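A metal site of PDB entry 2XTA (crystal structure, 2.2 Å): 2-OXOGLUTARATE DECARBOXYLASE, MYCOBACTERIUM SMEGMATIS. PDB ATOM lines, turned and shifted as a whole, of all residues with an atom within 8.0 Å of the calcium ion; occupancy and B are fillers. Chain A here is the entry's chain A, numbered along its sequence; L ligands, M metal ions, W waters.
Within 4 Å of the calcium ion: Asp 645, His 696, Asp 699 and Ile 701. The nearest printed residue that does not touch the calcium ion is Gln 702 (4.5 Å).
Water W1 bridges the side-chain carboxylate (OD2) of Asp 699 (3.2 Å) and a ring nitrogen (ND1) of His 696 (3.3 Å).
The side-chain carboxylate of Asp 645 sits close to the backbone NH of Arg 703, 3.4 Å away. OD2 of Asp 645 sits at hydrogen-bond distance from NE2 of Gln 702.
The side-chain hydroxyl (OG1) of Thr 679 sits at hydrogen-bond distance from a nitrogen (N3) of the ligand (3.2 Å). The guanidinium group of Arg 695 sits at hydrogen-bond distance from an oxygen (O1) of the ligand (2.9 Å).
The calcium ion is bound by OD1 of Asp 645 (2.4 Å). O of Ile 701 is bound to the calcium ion (2.5 Å). O of His 696 binds the calcium ion. The calcium ion is bound by OD1 of Asp 699, 2.7 Å away. The calcium ion has four donor atoms within binding distance. Slightly farther from the calcium ion lies OD2 of Asp 645 (2.9 Å). Slightly farther from the calcium ion lies water W1 (2.9 Å).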
ATOM      1  N   LYS A 535      -5.555 -25.483 -17.135  1.00  0.00           N
ATOM      2  CA  LYS A 535      -5.004 -24.276 -16.514  1.00  0.00           C
ATOM      3  C   LYS A 535      -3.919 -24.584 -15.477  1.00  0.00           C
ATOM      4  O   LYS A 535      -3.997 -25.593 -14.765  1.00  0.00           O
ATOM      5  CB  LYS A 535      -6.117 -23.449 -15.842  1.00  0.00           C
ATOM      6  CG  LYS A 535      -5.744 -21.987 -15.697  1.00  0.00           C
ATOM      7  CD  LYS A 535      -6.935 -21.090 -15.757  1.00  0.00           C
ATOM      8  CE  LYS A 535      -6.497 -19.669 -15.709  1.00  0.00           C
ATOM      9  NZ  LYS A 535      -6.412 -19.085 -17.064  1.00  0.00           N
ATOM     10  N   PRO A 608       0.196 -14.533 -17.792  1.00  0.00           N
ATOM     11  CA  PRO A 608      -1.207 -14.074 -17.757  1.00  0.00           C
ATOM     12  C   PRO A 608      -2.243 -15.203 -17.804  1.00  0.00           C
ATOM     13  O   PRO A 608      -3.394 -14.958 -17.435  1.00  0.00           O
ATOM     14  CB  PRO A 608      -1.338 -13.211 -19.028  1.00  0.00           C
ATOM     15  CG  PRO A 608       0.063 -12.832 -19.375  1.00  0.00           C
ATOM     16  CD  PRO A 608       0.886 -14.007 -18.990  1.00  0.00           C
ATOM     17  N   ALA A 610      -1.993 -18.088 -16.139  1.00  0.00           N
ATOM     18  CA  ALA A 610      -2.006 -18.802 -14.861  1.00  0.00           C
ATOM     19  C   ALA A 610      -3.085 -18.281 -13.936  1.00  0.00           C
ATOM     20  O   ALA A 610      -3.469 -17.108 -14.005  1.00  0.00           O
ATOM     21  CB  ALA A 610      -0.651 -18.687 -14.182  1.00  0.00           C
ATOM     22  N   MET A 611      -3.620 -19.179 -13.082  1.00  0.00           N
ATOM     23  CA  MET A 611      -4.558 -18.855 -12.002  1.00  0.00           C
ATOM     24  C   MET A 611      -3.643 -18.698 -10.805  1.00  0.00           C
ATOM     25  O   MET A 611      -2.984 -19.663 -10.451  1.00  0.00           O
ATOM     26  CB  MET A 611      -5.649 -19.945 -11.851  1.00  0.00           C
ATOM     27  CG  MET A 611      -6.620 -19.719 -10.683  1.00  0.00           C
ATOM     28  SD  MET A 611      -8.001 -18.606 -11.044  1.00  0.00           S
ATOM     29  CE  MET A 611      -8.826 -18.633  -9.473  1.00  0.00           C
ATOM     30  N   SER A 644      -2.667  -7.485 -14.293  1.00  0.00           N
ATOM     31  CA  SER A 644      -2.479  -8.569 -13.339  1.00  0.00           C
ATOM     32  C   SER A 644      -3.795  -9.212 -12.993  1.00  0.00           C
ATOM     33  O   SER A 644      -4.743  -8.502 -12.674  1.00  0.00           O
ATOM     34  CB  SER A 644      -1.827  -8.080 -12.064  1.00  0.00           C
ATOM     35  OG  SER A 644      -1.758  -9.121 -11.103  1.00  0.00           O
ATOM     36  N   ASP A 645      -3.826 -10.535 -13.002  1.00  0.00           N
ATOM     37  CA  ASP A 645      -4.985 -11.365 -12.680  1.00  0.00           C
ATOM     38  C   ASP A 645      -4.855 -11.971 -11.259  1.00  0.00           C
ATOM     39  O   ASP A 645      -5.552 -12.928 -10.940  1.00  0.00           O
ATOM     40  CB  ASP A 645      -5.095 -12.477 -13.737  1.00  0.00           C
ATOM     41  CG  ASP A 645      -6.507 -12.901 -14.032  1.00  0.00           C
ATOM     42  OD1 ASP A 645      -7.406 -12.031 -13.946  1.00  0.00           O
ATOM     43  OD2 ASP A 645      -6.709 -14.085 -14.384  1.00  0.00           O
ATOM     44  N   VAL A 646      -3.948 -11.443 -10.426  1.00  0.00           N
ATOM     45  CA  VAL A 646      -3.676 -12.002  -9.101  1.00  0.00           C
ATOM     46  C   VAL A 646      -4.940 -12.026  -8.198  1.00  0.00           C
ATOM     47  O   VAL A 646      -5.760 -11.110  -8.241  1.00  0.00           O
ATOM     48  CB  VAL A 646      -2.470 -11.293  -8.414  1.00  0.00           C
ATOM     49  CG1 VAL A 646      -2.814  -9.883  -7.935  1.00  0.00           C
ATOM     50  CG2 VAL A 646      -1.882 -12.144  -7.281  1.00  0.00           C
ATOM     51  N   VAL A 647      -5.079 -13.091  -7.411  1.00  0.00           N
ATOM     52  CA  VAL A 647      -6.173 -13.277  -6.451  1.00  0.00           C
ATOM     53  C   VAL A 647      -5.604 -13.144  -5.048  1.00  0.00           C
ATOM     54  O   VAL A 647      -4.617 -13.798  -4.728  1.00  0.00           O
ATOM     55  CB  VAL A 647      -6.917 -14.652  -6.595  1.00  0.00           C
ATOM     56  CG1 VAL A 647      -8.139 -14.740  -5.666  1.00  0.00           C
ATOM     57  CG2 VAL A 647      -7.312 -14.931  -8.044  1.00  0.00           C
ATOM     58  N   THR A 679     -11.857  -6.680  -8.909  1.00  0.00           N
ATOM     59  CA  THR A 679     -13.130  -7.283  -8.471  1.00  0.00           C
ATOM     60  C   THR A 679     -12.982  -7.480  -6.984  1.00  0.00           C
ATOM     61  O   THR A 679     -11.930  -7.958  -6.547  1.00  0.00           O
ATOM     62  CB  THR A 679     -13.494  -8.566  -9.248  1.00  0.00           C
ATOM     63  OG1 THR A 679     -13.508  -8.260 -10.645  1.00  0.00           O
ATOM     64  CG2 THR A 679     -14.867  -9.131  -8.845  1.00  0.00           C
ATOM     65  N   LEU A 692     -17.244 -17.874  -8.568  1.00  0.00           N
ATOM     66  CA  LEU A 692     -16.412 -16.662  -8.554  1.00  0.00           C
ATOM     67  C   LEU A 692     -14.979 -16.978  -9.037  1.00  0.00           C
ATOM     68  O   LEU A 692     -14.445 -16.244  -9.861  1.00  0.00           O
ATOM     69  CB  LEU A 692     -16.372 -16.047  -7.118  1.00  0.00           C
ATOM     70  CG  LEU A 692     -15.506 -14.765  -6.937  1.00  0.00           C
ATOM     71  CD1 LEU A 692     -16.236 -13.514  -7.451  1.00  0.00           C
ATOM     72  CD2 LEU A 692     -15.072 -14.608  -5.508  1.00  0.00           C
ATOM     73  N   LEU A 693     -14.364 -18.069  -8.520  1.00  0.00           N
ATOM     74  CA  LEU A 693     -12.995 -18.469  -8.892  1.00  0.00           C
ATOM     75  C   LEU A 693     -12.940 -18.954 -10.347  1.00  0.00           C
ATOM     76  O   LEU A 693     -12.002 -18.608 -11.076  1.00  0.00           O
ATOM     77  CB  LEU A 693     -12.437 -19.570  -7.968  1.00  0.00           C
ATOM     78  CG  LEU A 693     -12.167 -19.207  -6.506  1.00  0.00           C
ATOM     79  CD1 LEU A 693     -11.704 -20.447  -5.723  1.00  0.00           C
ATOM     80  CD2 LEU A 693     -11.140 -18.084  -6.385  1.00  0.00           C
ATOM     81  N   ARG A 694     -13.939 -19.733 -10.782  1.00  0.00           N
ATOM     82  CA  ARG A 694     -13.975 -20.235 -12.156  1.00  0.00           C
ATOM     83  C   ARG A 694     -14.202 -19.097 -13.156  1.00  0.00           C
ATOM     84  O   ARG A 694     -13.544 -19.091 -14.200  1.00  0.00           O
ATOM     85  CB  ARG A 694     -14.995 -21.357 -12.318  1.00  0.00           C
ATOM     86  CG  ARG A 694     -14.414 -22.683 -11.843  1.00  0.00           C
ATOM     87  CD  ARG A 694     -15.319 -23.893 -12.055  1.00  0.00           C
ATOM     88  NE  ARG A 694     -15.809 -24.057 -13.430  1.00  0.00           N
ATOM     89  CZ  ARG A 694     -15.084 -24.519 -14.440  1.00  0.00           C
ATOM     90  NH1 ARG A 694     -13.812 -24.849 -14.260  1.00  0.00           N
ATOM     91  NH2 ARG A 694     -15.616 -24.629 -15.650  1.00  0.00           N
ATOM     92  N   ARG A 695     -15.089 -18.105 -12.842  1.00  0.00           N
ATOM     93  CA  ARG A 695     -15.322 -16.952 -13.722  1.00  0.00           C
ATOM     94  C   ARG A 695     -14.001 -16.184 -13.864  1.00  0.00           C
ATOM     95  O   ARG A 695     -13.579 -15.920 -14.975  1.00  0.00           O
ATOM     96  CB  ARG A 695     -16.459 -16.032 -13.194  1.00  0.00           C
ATOM     97  CG  ARG A 695     -16.786 -14.825 -14.116  1.00  0.00           C
ATOM     98  CD  ARG A 695     -17.854 -13.892 -13.530  1.00  0.00           C
ATOM     99  NE  ARG A 695     -17.372 -13.171 -12.340  1.00  0.00           N
ATOM    100  CZ  ARG A 695     -18.055 -12.226 -11.689  1.00  0.00           C
ATOM    101  NH1 ARG A 695     -19.272 -11.882 -12.081  1.00  0.00           N
ATOM    102  NH2 ARG A 695     -17.529 -11.644 -10.621  1.00  0.00           N
ATOM    103  N   HIS A 696     -13.313 -15.924 -12.750  1.00  0.00           N
ATOM    104  CA  HIS A 696     -12.007 -15.232 -12.747  1.00  0.00           C
ATOM    105  C   HIS A 696     -10.965 -15.984 -13.568  1.00  0.00           C
ATOM    106  O   HIS A 696     -10.228 -15.355 -14.312  1.00  0.00           O
ATOM    107  CB  HIS A 696     -11.504 -15.023 -11.323  1.00  0.00           C
ATOM    108  CG  HIS A 696     -10.216 -14.235 -11.264  1.00  0.00           C
ATOM    109  ND1 HIS A 696     -10.191 -12.879 -11.502  1.00  0.00           N
ATOM    110  CD2 HIS A 696      -8.955 -14.666 -11.008  1.00  0.00           C
ATOM    111  CE1 HIS A 696      -8.923 -12.510 -11.364  1.00  0.00           C
ATOM    112  NE2 HIS A 696      -8.139 -13.555 -11.088  1.00  0.00           N
ATOM    113  N   GLY A 697     -10.936 -17.300 -13.444  1.00  0.00           N
ATOM    114  CA  GLY A 697      -9.988 -18.111 -14.198  1.00  0.00           C
ATOM    115  C   GLY A 697     -10.303 -18.276 -15.663  1.00  0.00           C
ATOM    116  O   GLY A 697      -9.414 -18.658 -16.428  1.00  0.00           O
ATOM    117  N   LYS A 698     -11.555 -18.009 -16.094  1.00  0.00           N
ATOM    118  CA  LYS A 698     -11.981 -18.258 -17.486  1.00  0.00           C
ATOM    119  C   LYS A 698     -12.465 -17.012 -18.275  1.00  0.00           C
ATOM    120  O   LYS A 698     -12.586 -17.118 -19.486  1.00  0.00           O
ATOM    121  CB  LYS A 698     -13.118 -19.303 -17.500  1.00  0.00           C
ATOM    122  CG  LYS A 698     -12.733 -20.689 -16.976  1.00  0.00           C
ATOM    123  CD  LYS A 698     -13.946 -21.587 -16.715  1.00  0.00           C
ATOM    124  CE  LYS A 698     -14.607 -22.132 -17.966  1.00  0.00           C
ATOM    125  NZ  LYS A 698     -13.672 -22.969 -18.784  1.00  0.00           N
ATOM    126  N   ASP A 699     -12.757 -15.880 -17.613  1.00  0.00           N
ATOM    127  CA  ASP A 699     -13.296 -14.660 -18.239  1.00  0.00           C
ATOM    128  C   ASP A 699     -12.309 -13.893 -19.162  1.00  0.00           C
ATOM    129  O   ASP A 699     -12.732 -13.004 -19.892  1.00  0.00           O
ATOM    130  CB  ASP A 699     -13.883 -13.694 -17.180  1.00  0.00           C
ATOM    131  CG  ASP A 699     -12.925 -13.130 -16.139  1.00  0.00           C
ATOM    132  OD1 ASP A 699     -11.684 -13.248 -16.346  1.00  0.00           O
ATOM    133  OD2 ASP A 699     -13.408 -12.577 -15.124  1.00  0.00           O
ATOM    134  N   GLY A 700     -11.011 -14.160 -19.045  1.00  0.00           N
ATOM    135  CA  GLY A 700     -10.015 -13.447 -19.854  1.00  0.00           C
ATOM    136  C   GLY A 700      -9.800 -11.989 -19.495  1.00  0.00           C
ATOM    137  O   GLY A 700      -9.118 -11.274 -20.232  1.00  0.00           O
ATOM    138  N   ILE A 701     -10.406 -11.508 -18.393  1.00  0.00           N
ATOM    139  CA  ILE A 701     -10.272 -10.137 -17.871  1.00  0.00           C
ATOM    140  C   ILE A 701      -9.059 -10.149 -16.922  1.00  0.00           C
ATOM    141  O   ILE A 701      -9.163 -10.726 -15.831  1.00  0.00           O
ATOM    142  CB  ILE A 701     -11.582  -9.655 -17.170  1.00  0.00           C
ATOM    143  CG1 ILE A 701     -12.757  -9.571 -18.181  1.00  0.00           C
ATOM    144  CG2 ILE A 701     -11.385  -8.309 -16.456  1.00  0.00           C
ATOM    145  CD1 ILE A 701     -14.130  -9.654 -17.558  1.00  0.00           C
ATOM    146  N   GLN A 702      -7.923  -9.578 -17.349  1.00  0.00           N
ATOM    147  CA  GLN A 702      -6.702  -9.530 -16.537  1.00  0.00           C
ATOM    148  C   GLN A 702      -6.789  -8.407 -15.507  1.00  0.00           C
ATOM    149  O   GLN A 702      -6.174  -7.345 -15.688  1.00  0.00           O
ATOM    150  CB  GLN A 702      -5.442  -9.410 -17.417  1.00  0.00           C
ATOM    151  CG  GLN A 702      -5.104 -10.640 -18.235  1.00  0.00           C
ATOM    152  CD  GLN A 702      -4.738 -11.822 -17.395  1.00  0.00           C
ATOM    153  OE1 GLN A 702      -3.680 -11.856 -16.763  1.00  0.00           O
ATOM    154  NE2 GLN A 702      -5.595 -12.845 -17.390  1.00  0.00           N
ATOM    155  N   ARG A 703      -7.551  -8.634 -14.419  1.00  0.00           N
ATOM    156  CA  ARG A 703      -7.714  -7.652 -13.329  1.00  0.00           C
ATOM    157  C   ARG A 703      -7.718  -8.367 -11.999  1.00  0.00           C
ATOM    158  O   ARG A 703      -8.210  -9.479 -11.907  1.00  0.00           O
ATOM    159  CB  ARG A 703      -8.980  -6.814 -13.521  1.00  0.00           C
ATOM    160  CG  ARG A 703      -8.723  -5.682 -14.501  1.00  0.00           C
ATOM    161  CD  ARG A 703      -9.962  -4.995 -14.970  1.00  0.00           C
ATOM    162  NE  ARG A 703      -9.603  -3.947 -15.936  1.00  0.00           N
ATOM    163  CZ  ARG A 703     -10.462  -3.328 -16.737  1.00  0.00           C
ATOM    164  NH1 ARG A 703     -11.759  -3.629 -16.694  1.00  0.00           N
ATOM    165  NH2 ARG A 703     -10.028  -2.431 -17.608  1.00  0.00           N
ATOM    166  N   PRO A 704      -7.136  -7.781 -10.921  1.00  0.00           N
ATOM    167  CA  PRO A 704      -7.074  -8.501  -9.640  1.00  0.00           C
ATOM    168  C   PRO A 704      -8.435  -8.820  -9.023  1.00  0.00           C
ATOM    169  O   PRO A 704      -9.421  -8.130  -9.296  1.00  0.00           O
ATOM    170  CB  PRO A 704      -6.277  -7.557  -8.741  1.00  0.00           C
ATOM    171  CG  PRO A 704      -5.504  -6.693  -9.700  1.00  0.00           C
ATOM    172  CD  PRO A 704      -6.416  -6.477 -10.843  1.00  0.00           C
ATOM    173  N   LEU A 705      -8.495  -9.900  -8.223  1.00  0.00           N
ATOM    174  CA  LEU A 705      -9.681 -10.335  -7.522  1.00  0.00           C
ATOM    175  C   LEU A 705      -9.371 -10.341  -6.022  1.00  0.00           C
ATOM    176  O   LEU A 705      -8.422 -10.983  -5.590  1.00  0.00           O
ATOM    177  CB  LEU A 705     -10.161 -11.722  -8.012  1.00  0.00           C
ATOM    178  CG  LEU A 705     -11.269 -12.428  -7.191  1.00  0.00           C
ATOM    179  CD1 LEU A 705     -12.636 -11.766  -7.389  1.00  0.00           C
ATOM    180  CD2 LEU A 705     -11.379 -13.876  -7.584  1.00  0.00           C
HETATM  181  N1  LIG L   1     -15.864  -9.622 -13.654  1.00  0.00           N
HETATM  182  C1  LIG L   1     -16.216 -10.388 -14.704  1.00  0.00           C
HETATM  183  N2  LIG L   1     -17.510 -10.468 -15.075  1.00  0.00           N
HETATM  184  C2  LIG L   1     -18.489  -9.756 -14.445  1.00  0.00           C
HETATM  185  C3  LIG L   1     -18.151  -8.918 -13.360  1.00  0.00           C
HETATM  186  C4  LIG L   1     -16.776  -8.867 -12.979  1.00  0.00           C
HETATM  187  N3  LIG L   1     -16.407  -8.078 -11.918  1.00  0.00           N
HETATM  188  N4  LIG L   1     -19.297  -8.333 -12.908  1.00  0.00           N
HETATM  189  C5  LIG L   1     -20.303  -8.722 -13.646  1.00  0.00           C
HETATM  190  N5  LIG L   1     -19.847  -9.605 -14.603  1.00  0.00           N
HETATM  191  C6  LIG L   1     -20.651 -10.296 -15.599  1.00  0.00           C
HETATM  192  C7  LIG L   1     -21.481 -11.318 -14.765  1.00  0.00           C
HETATM  193  O1  LIG L   1     -20.785 -12.533 -14.447  1.00  0.00           O
HETATM  194  C8  LIG L   1     -22.742 -11.490 -15.643  1.00  0.00           C
HETATM  195  O2  LIG L   1     -22.484 -12.395 -16.737  1.00  0.00           O
HETATM  196  P1  LIG L   1     -23.906 -13.021 -17.297  1.00  0.00           P
HETATM  197  O3  LIG L   1     -23.806 -14.651 -17.189  1.00  0.00           O
HETATM  198  O4  LIG L   1     -25.194 -12.641 -16.402  1.00  0.00           O
HETATM  199  O5  LIG L   1     -24.119 -12.520 -18.665  1.00  0.00           O
HETATM  200  C9  LIG L   1     -22.915 -10.056 -16.224  1.00  0.00           C
HETATM  201  O6  LIG L   1     -21.630  -9.397 -16.211  1.00  0.00           O
HETATM  202  C10 LIG L   1     -23.973  -9.286 -15.430  1.00  0.00           C
HETATM  203  O7  LIG L   1     -23.459  -9.030 -14.114  1.00  0.00           O
HETATM  204  P2  LIG L   1     -24.554  -9.141 -12.912  1.00  0.00           P
HETATM  205  O8  LIG L   1     -25.875 -10.003 -13.332  1.00  0.00           O
HETATM  206  O9  LIG L   1     -23.852  -9.819 -11.790  1.00  0.00           O
HETATM  207  O10 LIG L   1     -24.987  -7.694 -12.290  1.00  0.00           O
HETATM  208  P3  LIG L   1     -25.167  -6.363 -13.248  1.00  0.00           P
HETATM  209  O11 LIG L   1     -25.933  -5.397 -12.222  1.00  0.00           O
HETATM  210  O12 LIG L   1     -25.912  -6.637 -14.532  1.00  0.00           O
HETATM  211  O13 LIG L   1     -23.661  -5.691 -13.590  1.00  0.00           O
HETATM  212  C11 LIG L   1     -22.209  -3.827 -14.110  1.00  0.00           C
HETATM  213  C12 LIG L   1     -23.682  -4.292 -13.946  1.00  0.00           C
HETATM  214 CA    CA M   1      -9.376 -13.023 -14.934  1.00  0.00          CA
HETATM  215  O   HOH W   1     -10.985 -10.793 -13.898  1.00  0.00           O
